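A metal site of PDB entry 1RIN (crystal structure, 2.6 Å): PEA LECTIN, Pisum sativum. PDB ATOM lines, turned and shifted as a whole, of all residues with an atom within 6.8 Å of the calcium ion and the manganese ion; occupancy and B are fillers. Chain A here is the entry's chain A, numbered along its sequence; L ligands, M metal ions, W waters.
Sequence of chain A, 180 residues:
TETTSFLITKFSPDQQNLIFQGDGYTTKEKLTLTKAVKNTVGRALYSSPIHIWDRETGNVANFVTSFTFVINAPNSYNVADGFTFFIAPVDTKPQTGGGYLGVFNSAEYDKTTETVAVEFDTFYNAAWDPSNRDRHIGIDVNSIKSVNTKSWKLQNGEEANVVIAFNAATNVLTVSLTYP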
ATOM      1  N   ASP A  81      -9.195 -21.580  -6.705  1.00  0.00           N
ATOM      2  CA  ASP A  81      -9.798 -22.622  -7.496  1.00  0.00           C
ATOM      3  C   ASP A  81      -9.946 -23.938  -6.761  1.00  0.00           C
ATOM      4  O   ASP A  81     -10.884 -24.720  -6.973  1.00  0.00           O
ATOM      5  CB  ASP A  81      -8.983 -22.856  -8.661  1.00  0.00           C
ATOM      6  CG  ASP A  81      -9.594 -21.995  -9.757  1.00  0.00           C
ATOM      7  OD1 ASP A  81     -10.528 -22.392 -10.410  1.00  0.00           O
ATOM      8  OD2 ASP A  81      -9.143 -20.872 -10.002  1.00  0.00           O
ATOM      9  N   GLY A  98      -5.393 -22.323 -12.769  1.00  0.00           N
ATOM     10  CA  GLY A  98      -6.772 -21.932 -12.568  1.00  0.00           C
ATOM     11  C   GLY A  98      -7.710 -23.115 -12.352  1.00  0.00           C
ATOM     12  O   GLY A  98      -7.505 -23.963 -11.477  1.00  0.00           O
ATOM     13  N   GLY A  99      -8.673 -23.315 -13.238  1.00  0.00           N
ATOM     14  CA  GLY A  99      -9.661 -24.354 -13.061  1.00  0.00           C
ATOM     15  C   GLY A  99      -9.120 -25.752 -13.172  1.00  0.00           C
ATOM     16  O   GLY A  99      -9.800 -26.686 -12.787  1.00  0.00           O
ATOM     17  N   TYR A 100      -7.907 -25.945 -13.705  1.00  0.00           N
ATOM     18  CA  TYR A 100      -7.346 -27.307 -13.846  1.00  0.00           C
ATOM     19  C   TYR A 100      -6.484 -27.771 -12.685  1.00  0.00           C
ATOM     20  O   TYR A 100      -5.830 -28.820 -12.728  1.00  0.00           O
ATOM     21  CB  TYR A 100      -6.525 -27.420 -15.111  1.00  0.00           C
ATOM     22  CG  TYR A 100      -7.380 -27.246 -16.349  1.00  0.00           C
ATOM     23  CD1 TYR A 100      -8.094 -28.311 -16.848  1.00  0.00           C
ATOM     24  CD2 TYR A 100      -7.431 -26.024 -16.955  1.00  0.00           C
ATOM     25  CE1 TYR A 100      -8.871 -28.163 -17.964  1.00  0.00           C
ATOM     26  CE2 TYR A 100      -8.204 -25.868 -18.081  1.00  0.00           C
ATOM     27  CZ  TYR A 100      -8.917 -26.933 -18.581  1.00  0.00           C
ATOM     28  OH  TYR A 100      -9.700 -26.772 -19.699  1.00  0.00           O
ATOM     29  N   LEU A 101      -6.467 -26.971 -11.616  1.00  0.00           N
ATOM     30  CA  LEU A 101      -5.833 -27.294 -10.334  1.00  0.00           C
ATOM     31  C   LEU A 101      -4.340 -27.641 -10.366  1.00  0.00           C
ATOM     32  O   LEU A 101      -3.730 -28.004  -9.347  1.00  0.00           O
ATOM     33  CB  LEU A 101      -6.662 -28.441  -9.659  1.00  0.00           C
ATOM     34  CG  LEU A 101      -8.186 -28.206  -9.492  1.00  0.00           C
ATOM     35  CD1 LEU A 101      -8.874 -29.411  -8.899  1.00  0.00           C
ATOM     36  CD2 LEU A 101      -8.419 -27.018  -8.586  1.00  0.00           C
ATOM     37  N   GLU A 119      -9.830 -34.009  -5.664  1.00  0.00           N
ATOM     38  CA  GLU A 119      -9.942 -32.557  -5.597  1.00  0.00           C
ATOM     39  C   GLU A 119     -10.896 -32.026  -4.549  1.00  0.00           C
ATOM     40  O   GLU A 119     -11.840 -32.698  -4.133  1.00  0.00           O
ATOM     41  CB  GLU A 119     -10.375 -31.999  -6.910  1.00  0.00           C
ATOM     42  CG  GLU A 119     -11.762 -32.487  -7.315  1.00  0.00           C
ATOM     43  CD  GLU A 119     -12.335 -31.798  -8.527  1.00  0.00           C
ATOM     44  OE1 GLU A 119     -11.680 -31.778  -9.542  1.00  0.00           O
ATOM     45  OE2 GLU A 119     -13.438 -31.290  -8.436  1.00  0.00           O
ATOM     46  N   PHE A 120     -10.622 -30.822  -4.105  1.00  0.00           N
ATOM     47  CA  PHE A 120     -11.462 -30.071  -3.189  1.00  0.00           C
ATOM     48  C   PHE A 120     -11.662 -28.768  -3.958  1.00  0.00           C
ATOM     49  O   PHE A 120     -10.849 -27.828  -3.942  1.00  0.00           O
ATOM     50  CB  PHE A 120     -10.730 -29.863  -1.838  1.00  0.00           C
ATOM     51  CG  PHE A 120     -10.372 -31.203  -1.176  1.00  0.00           C
ATOM     52  CD1 PHE A 120     -11.292 -31.884  -0.395  1.00  0.00           C
ATOM     53  CD2 PHE A 120      -9.133 -31.779  -1.406  1.00  0.00           C
ATOM     54  CE1 PHE A 120     -10.962 -33.136   0.101  1.00  0.00           C
ATOM     55  CE2 PHE A 120      -8.826 -33.034  -0.911  1.00  0.00           C
ATOM     56  CZ  PHE A 120      -9.740 -33.714  -0.146  1.00  0.00           C
ATOM     57  N   ASP A 121     -12.707 -28.775  -4.766  1.00  0.00           N
ATOM     58  CA  ASP A 121     -12.961 -27.729  -5.741  1.00  0.00           C
ATOM     59  C   ASP A 121     -13.915 -26.655  -5.219  1.00  0.00           C
ATOM     60  O   ASP A 121     -15.077 -26.895  -4.865  1.00  0.00           O
ATOM     61  CB  ASP A 121     -13.507 -28.417  -6.986  1.00  0.00           C
ATOM     62  CG  ASP A 121     -13.675 -27.610  -8.268  1.00  0.00           C
ATOM     63  OD1 ASP A 121     -13.786 -26.383  -8.196  1.00  0.00           O
ATOM     64  OD2 ASP A 121     -13.695 -28.196  -9.362  1.00  0.00           O
ATOM     65  N   THR A 122     -13.417 -25.411  -5.206  1.00  0.00           N
ATOM     66  CA  THR A 122     -14.171 -24.283  -4.667  1.00  0.00           C
ATOM     67  C   THR A 122     -14.839 -23.370  -5.709  1.00  0.00           C
ATOM     68  O   THR A 122     -15.641 -22.486  -5.411  1.00  0.00           O
ATOM     69  CB  THR A 122     -13.283 -23.422  -3.791  1.00  0.00           C
ATOM     70  OG1 THR A 122     -12.167 -23.059  -4.571  1.00  0.00           O
ATOM     71  CG2 THR A 122     -12.785 -24.134  -2.561  1.00  0.00           C
ATOM     72  N   PHE A 123     -14.594 -23.652  -6.990  1.00  0.00           N
ATOM     73  CA  PHE A 123     -15.061 -22.800  -8.046  1.00  0.00           C
ATOM     74  C   PHE A 123     -15.751 -23.576  -9.125  1.00  0.00           C
ATOM     75  O   PHE A 123     -15.191 -24.534  -9.665  1.00  0.00           O
ATOM     76  CB  PHE A 123     -13.903 -22.047  -8.690  1.00  0.00           C
ATOM     77  CG  PHE A 123     -14.356 -20.948  -9.656  1.00  0.00           C
ATOM     78  CD1 PHE A 123     -14.676 -19.693  -9.160  1.00  0.00           C
ATOM     79  CD2 PHE A 123     -14.406 -21.217 -11.013  1.00  0.00           C
ATOM     80  CE1 PHE A 123     -15.047 -18.685 -10.033  1.00  0.00           C
ATOM     81  CE2 PHE A 123     -14.780 -20.226 -11.881  1.00  0.00           C
ATOM     82  CZ  PHE A 123     -15.113 -18.969 -11.389  1.00  0.00           C
ATOM     83  N   TYR A 124     -16.960 -23.120  -9.506  1.00  0.00           N
ATOM     84  CA  TYR A 124     -17.725 -23.806 -10.536  1.00  0.00           C
ATOM     85  C   TYR A 124     -17.219 -23.405 -11.912  1.00  0.00           C
ATOM     86  O   TYR A 124     -17.202 -22.240 -12.302  1.00  0.00           O
ATOM     87  CB  TYR A 124     -19.250 -23.469 -10.357  1.00  0.00           C
ATOM     88  CG  TYR A 124     -20.138 -24.012 -11.475  1.00  0.00           C
ATOM     89  CD1 TYR A 124     -20.393 -25.373 -11.604  1.00  0.00           C
ATOM     90  CD2 TYR A 124     -20.624 -23.120 -12.416  1.00  0.00           C
ATOM     91  CE1 TYR A 124     -21.126 -25.818 -12.690  1.00  0.00           C
ATOM     92  CE2 TYR A 124     -21.358 -23.566 -13.501  1.00  0.00           C
ATOM     93  CZ  TYR A 124     -21.592 -24.908 -13.618  1.00  0.00           C
ATOM     94  OH  TYR A 124     -22.296 -25.327 -14.719  1.00  0.00           O
ATOM     95  N   ASN A 125     -16.786 -24.387 -12.668  1.00  0.00           N
ATOM     96  CA  ASN A 125     -16.388 -24.198 -14.043  1.00  0.00           C
ATOM     97  C   ASN A 125     -17.425 -24.897 -14.900  1.00  0.00           C
ATOM     98  O   ASN A 125     -17.506 -26.134 -14.979  1.00  0.00           O
ATOM     99  CB  ASN A 125     -15.023 -24.823 -14.354  1.00  0.00           C
ATOM    100  CG  ASN A 125     -13.870 -24.208 -13.581  1.00  0.00           C
ATOM    101  OD1 ASN A 125     -13.442 -24.818 -12.615  1.00  0.00           O
ATOM    102  ND2 ASN A 125     -13.275 -23.066 -13.877  1.00  0.00           N
ATOM    103  N   TRP A 128     -17.271 -28.515 -17.023  1.00  0.00           N
ATOM    104  CA  TRP A 128     -17.063 -29.877 -16.482  1.00  0.00           C
ATOM    105  C   TRP A 128     -17.521 -30.043 -15.029  1.00  0.00           C
ATOM    106  O   TRP A 128     -17.739 -31.158 -14.576  1.00  0.00           O
ATOM    107  CB  TRP A 128     -15.562 -30.281 -16.554  1.00  0.00           C
ATOM    108  CG  TRP A 128     -14.590 -29.315 -15.863  1.00  0.00           C
ATOM    109  CD1 TRP A 128     -14.524 -29.289 -14.507  1.00  0.00           C
ATOM    110  CD2 TRP A 128     -13.778 -28.349 -16.441  1.00  0.00           C
ATOM    111  NE1 TRP A 128     -13.718 -28.319 -14.203  1.00  0.00           N
ATOM    112  CE2 TRP A 128     -13.250 -27.725 -15.318  1.00  0.00           C
ATOM    113  CE3 TRP A 128     -13.416 -27.878 -17.700  1.00  0.00           C
ATOM    114  CZ2 TRP A 128     -12.362 -26.668 -15.435  1.00  0.00           C
ATOM    115  CZ3 TRP A 128     -12.528 -26.821 -17.817  1.00  0.00           C
ATOM    116  CH2 TRP A 128     -12.011 -26.225 -16.691  1.00  0.00           C
ATOM    117  N   ASP A 129     -17.701 -28.945 -14.264  1.00  0.00           N
ATOM    118  CA  ASP A 129     -18.106 -29.072 -12.873  1.00  0.00           C
ATOM    119  C   ASP A 129     -19.594 -29.362 -12.654  1.00  0.00           C
ATOM    120  O   ASP A 129     -20.418 -28.943 -13.481  1.00  0.00           O
ATOM    121  CB  ASP A 129     -17.696 -27.810 -12.118  1.00  0.00           C
ATOM    122  CG  ASP A 129     -16.236 -27.808 -11.674  1.00  0.00           C
ATOM    123  OD1 ASP A 129     -15.632 -28.859 -11.514  1.00  0.00           O
ATOM    124  OD2 ASP A 129     -15.681 -26.735 -11.443  1.00  0.00           O
ATOM    125  N   PRO A 130     -19.997 -30.013 -11.549  1.00  0.00           N
ATOM    126  CA  PRO A 130     -21.388 -30.365 -11.257  1.00  0.00           C
ATOM    127  C   PRO A 130     -22.411 -29.262 -11.417  1.00  0.00           C
ATOM    128  O   PRO A 130     -22.279 -28.139 -10.922  1.00  0.00           O
ATOM    129  CB  PRO A 130     -21.391 -30.888  -9.853  1.00  0.00           C
ATOM    130  CG  PRO A 130     -19.989 -31.315  -9.599  1.00  0.00           C
ATOM    131  CD  PRO A 130     -19.196 -30.256 -10.347  1.00  0.00           C
ATOM    132  N   HIS A 136     -17.343 -28.866  -4.041  1.00  0.00           N
ATOM    133  CA  HIS A 136     -17.443 -30.299  -3.951  1.00  0.00           C
ATOM    134  C   HIS A 136     -16.129 -31.011  -3.781  1.00  0.00           C
ATOM    135  O   HIS A 136     -15.046 -30.488  -4.044  1.00  0.00           O
ATOM    136  CB  HIS A 136     -18.172 -30.825  -5.236  1.00  0.00           C
ATOM    137  CG  HIS A 136     -17.502 -30.393  -6.536  1.00  0.00           C
ATOM    138  ND1 HIS A 136     -17.678 -29.204  -7.085  1.00  0.00           N
ATOM    139  CD2 HIS A 136     -16.580 -31.106  -7.279  1.00  0.00           C
ATOM    140  CE1 HIS A 136     -16.895 -29.121  -8.112  1.00  0.00           C
ATOM    141  NE2 HIS A 136     -16.239 -30.273  -8.234  1.00  0.00           N
ATOM    142  N   ILE A 137     -16.216 -32.226  -3.298  1.00  0.00           N
ATOM    143  CA  ILE A 137     -15.122 -33.175  -3.272  1.00  0.00           C
ATOM    144  C   ILE A 137     -15.238 -33.957  -4.561  1.00  0.00           C
ATOM    145  O   ILE A 137     -16.347 -34.132  -5.075  1.00  0.00           O
ATOM    146  CB  ILE A 137     -15.256 -34.113  -2.057  1.00  0.00           C
ATOM    147  CG1 ILE A 137     -15.188 -33.306  -0.777  1.00  0.00           C
ATOM    148  CG2 ILE A 137     -14.113 -35.107  -2.010  1.00  0.00           C
ATOM    149  CD1 ILE A 137     -15.514 -34.120   0.486  1.00  0.00           C
ATOM    150  N   GLY A 138     -14.149 -34.401  -5.147  1.00  0.00           N
ATOM    151  CA  GLY A 138     -14.243 -35.215  -6.351  1.00  0.00           C
ATOM    152  C   GLY A 138     -13.077 -36.175  -6.574  1.00  0.00           C
ATOM    153  O   GLY A 138     -11.950 -35.976  -6.109  1.00  0.00           O
ATOM    154  N   ASP A 140     -10.732 -37.645  -9.472  1.00  0.00           N
ATOM    155  CA  ASP A 140     -10.336 -37.395 -10.847  1.00  0.00           C
ATOM    156  C   ASP A 140      -9.362 -38.403 -11.460  1.00  0.00           C
ATOM    157  O   ASP A 140      -8.252 -38.641 -10.990  1.00  0.00           O
ATOM    158  CB  ASP A 140      -9.688 -36.019 -10.992  1.00  0.00           C
ATOM    159  CG  ASP A 140     -10.460 -34.762 -10.641  1.00  0.00           C
ATOM    160  OD1 ASP A 140     -11.663 -34.806 -10.433  1.00  0.00           O
ATOM    161  OD2 ASP A 140      -9.841 -33.701 -10.590  1.00  0.00           O
ATOM    162  N   ILE A 144     -10.062 -33.409 -15.795  1.00  0.00           N
ATOM    163  CA  ILE A 144     -10.497 -32.508 -14.731  1.00  0.00           C
ATOM    164  C   ILE A 144     -12.005 -32.675 -14.464  1.00  0.00           C
ATOM    165  O   ILE A 144     -12.574 -32.162 -13.504  1.00  0.00           O
ATOM    166  CB  ILE A 144     -10.118 -31.064 -15.131  1.00  0.00           C
ATOM    167  CG1 ILE A 144     -10.319 -30.140 -13.931  1.00  0.00           C
ATOM    168  CG2 ILE A 144     -10.926 -30.587 -16.317  1.00  0.00           C
ATOM    169  CD1 ILE A 144      -9.500 -30.493 -12.675  1.00  0.00           C
ATOM    170  N   LYS A 145     -12.671 -33.439 -15.311  1.00  0.00           N
ATOM    171  CA  LYS A 145     -14.056 -33.761 -15.096  1.00  0.00           C
ATOM    172  C   LYS A 145     -14.140 -35.015 -14.242  1.00  0.00           C
ATOM    173  O   LYS A 145     -13.904 -36.126 -14.716  1.00  0.00           O
ATOM    174  CB  LYS A 145     -14.740 -33.961 -16.432  1.00  0.00           C
ATOM    175  CG  LYS A 145     -16.233 -34.114 -16.232  1.00  0.00           C
ATOM    176  CD  LYS A 145     -16.894 -33.903 -17.553  1.00  0.00           C
ATOM    177  CE  LYS A 145     -17.773 -35.111 -17.761  1.00  0.00           C
ATOM    178  NZ  LYS A 145     -18.772 -34.830 -18.778  1.00  0.00           N
ATOM    179  N   SER A 146     -14.402 -34.827 -12.955  1.00  0.00           N
ATOM    180  CA  SER A 146     -14.407 -35.931 -12.003  1.00  0.00           C
ATOM    181  C   SER A 146     -15.316 -37.131 -12.281  1.00  0.00           C
ATOM    182  O   SER A 146     -16.492 -36.989 -12.664  1.00  0.00           O
ATOM    183  CB  SER A 146     -14.801 -35.490 -10.611  1.00  0.00           C
ATOM    184  OG  SER A 146     -14.440 -34.167 -10.266  1.00  0.00           O
ATOM    185  N   THR A 149     -18.392 -36.984  -7.549  1.00  0.00           N
ATOM    186  CA  THR A 149     -18.307 -35.799  -6.681  1.00  0.00           C
ATOM    187  C   THR A 149     -19.297 -35.798  -5.501  1.00  0.00           C
ATOM    188  O   THR A 149     -20.253 -36.578  -5.423  1.00  0.00           O
ATOM    189  CB  THR A 149     -18.594 -34.479  -7.386  1.00  0.00           C
ATOM    190  OG1 THR A 149     -19.957 -34.523  -7.770  1.00  0.00           O
ATOM    191  CG2 THR A 149     -17.686 -34.220  -8.568  1.00  0.00           C
HETATM  192  C1  LIG L   1     -10.788 -17.771 -14.635  1.00  0.00           C
HETATM  193  C2  LIG L   1      -9.966 -18.971 -15.128  1.00  0.00           C
HETATM  194  C3  LIG L   1     -10.580 -20.254 -14.602  1.00  0.00           C
HETATM  195  C4  LIG L   1     -10.627 -20.190 -13.113  1.00  0.00           C
HETATM  196  C5  LIG L   1     -11.395 -18.960 -12.688  1.00  0.00           C
HETATM  197  C6  LIG L   1     -11.442 -18.823 -11.181  1.00  0.00           C
HETATM  198  O1  LIG L   1     -12.125 -17.752 -15.155  1.00  0.00           O
HETATM  199  O2  LIG L   1      -8.597 -18.854 -14.743  1.00  0.00           O
HETATM  200  O3  LIG L   1      -9.883 -21.401 -15.038  1.00  0.00           O
HETATM  201  O4  LIG L   1     -11.268 -21.326 -12.626  1.00  0.00           O
HETATM  202  O5  LIG L   1     -10.778 -17.792 -13.207  1.00  0.00           O
HETATM  203  O6  LIG L   1     -10.229 -18.416 -10.626  1.00  0.00           O
HETATM  204 CA    CA M   1     -13.709 -26.029 -10.480  1.00  0.00          CA
HETATM  205 MN    MN M   2     -14.605 -30.073  -9.886  1.00  0.00          MN
HETATM  206  O   HOH W   1     -12.024 -24.574  -9.607  1.00  0.00           O
HETATM  207  O   HOH W   2     -12.401 -27.460 -11.946  1.00  0.00           O
HETATM  208  O   HOH W   3     -15.535 -31.818 -10.845  1.00  0.00           O
HETATM  209  O   HOH W   4     -13.077 -30.365 -11.246  1.00  0.00           O
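Four residues have an atom within 4 Å of the calcium ion: Asp 121, Phe 123, Asn 125 and Asp 129.
The manganese ion is bound by water W4 (2.1 Å), the side-chain carboxylate (OD2) of Asp 121 (2.2 Å), water W3 (2.2 Å), the side-chain carboxylate (OE2) of Glu 119 (2.2 Å), the side-chain carboxylate (OD1) of Asp 129 (2.3 Å) and a ring nitrogen (NE2) of His 136 (2.3 Å).
Within 4 Å of the manganese ion: Glu 119, Asp 121, Asp 129 and His 136.
O of Gly 138 lies within hydrogen-bond range of N of Glu 119 (2.9 Å).
OD1 of Asp 129 lies close to NE1 of Trp 128.
Water W2 bridges the indole nitrogen (NE1) of Trp 128 (2.8 Å) and the backbone carbonyl oxygen (O) of Gly 99 (2.8 Å).
Water W4 lies within hydrogen-bond range of the side-chain carboxylate (OE1) of Glu 119 (2.6 Å) and the backbone carbonyl oxygen (O) of Ile 144 (2.9 Å).
O of Phe 123 is bound to the calcium ion, at 2.3 Å.
The calcium ion is bound by the side-chain carboxylate (OD2) of Asp 129, 2.3 Å away.
OD1 of Asp 121 binds the calcium ion (2.3 Å).
Water W1 is bound to the calcium ion (2.4 Å).
The calcium ion is bound by water W2.
The calcium ion is bound by the side-chain carboxylate (OD2) of Asp 121 (2.4 Å).
The calcium ion is bound by OD1 of Asn 125 (2.5 Å).
The calcium ion has seven donor atoms within binding distance.
ND2 of Asn 125 lies within hydrogen-bond range of O4 of the ligand (2.9 Å).
OD1 of Asp 81 sits at hydrogen-bond distance from O4 of the ligand (2.6 Å).
O3 of the ligand lies within hydrogen-bond range of N of Gly 99.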
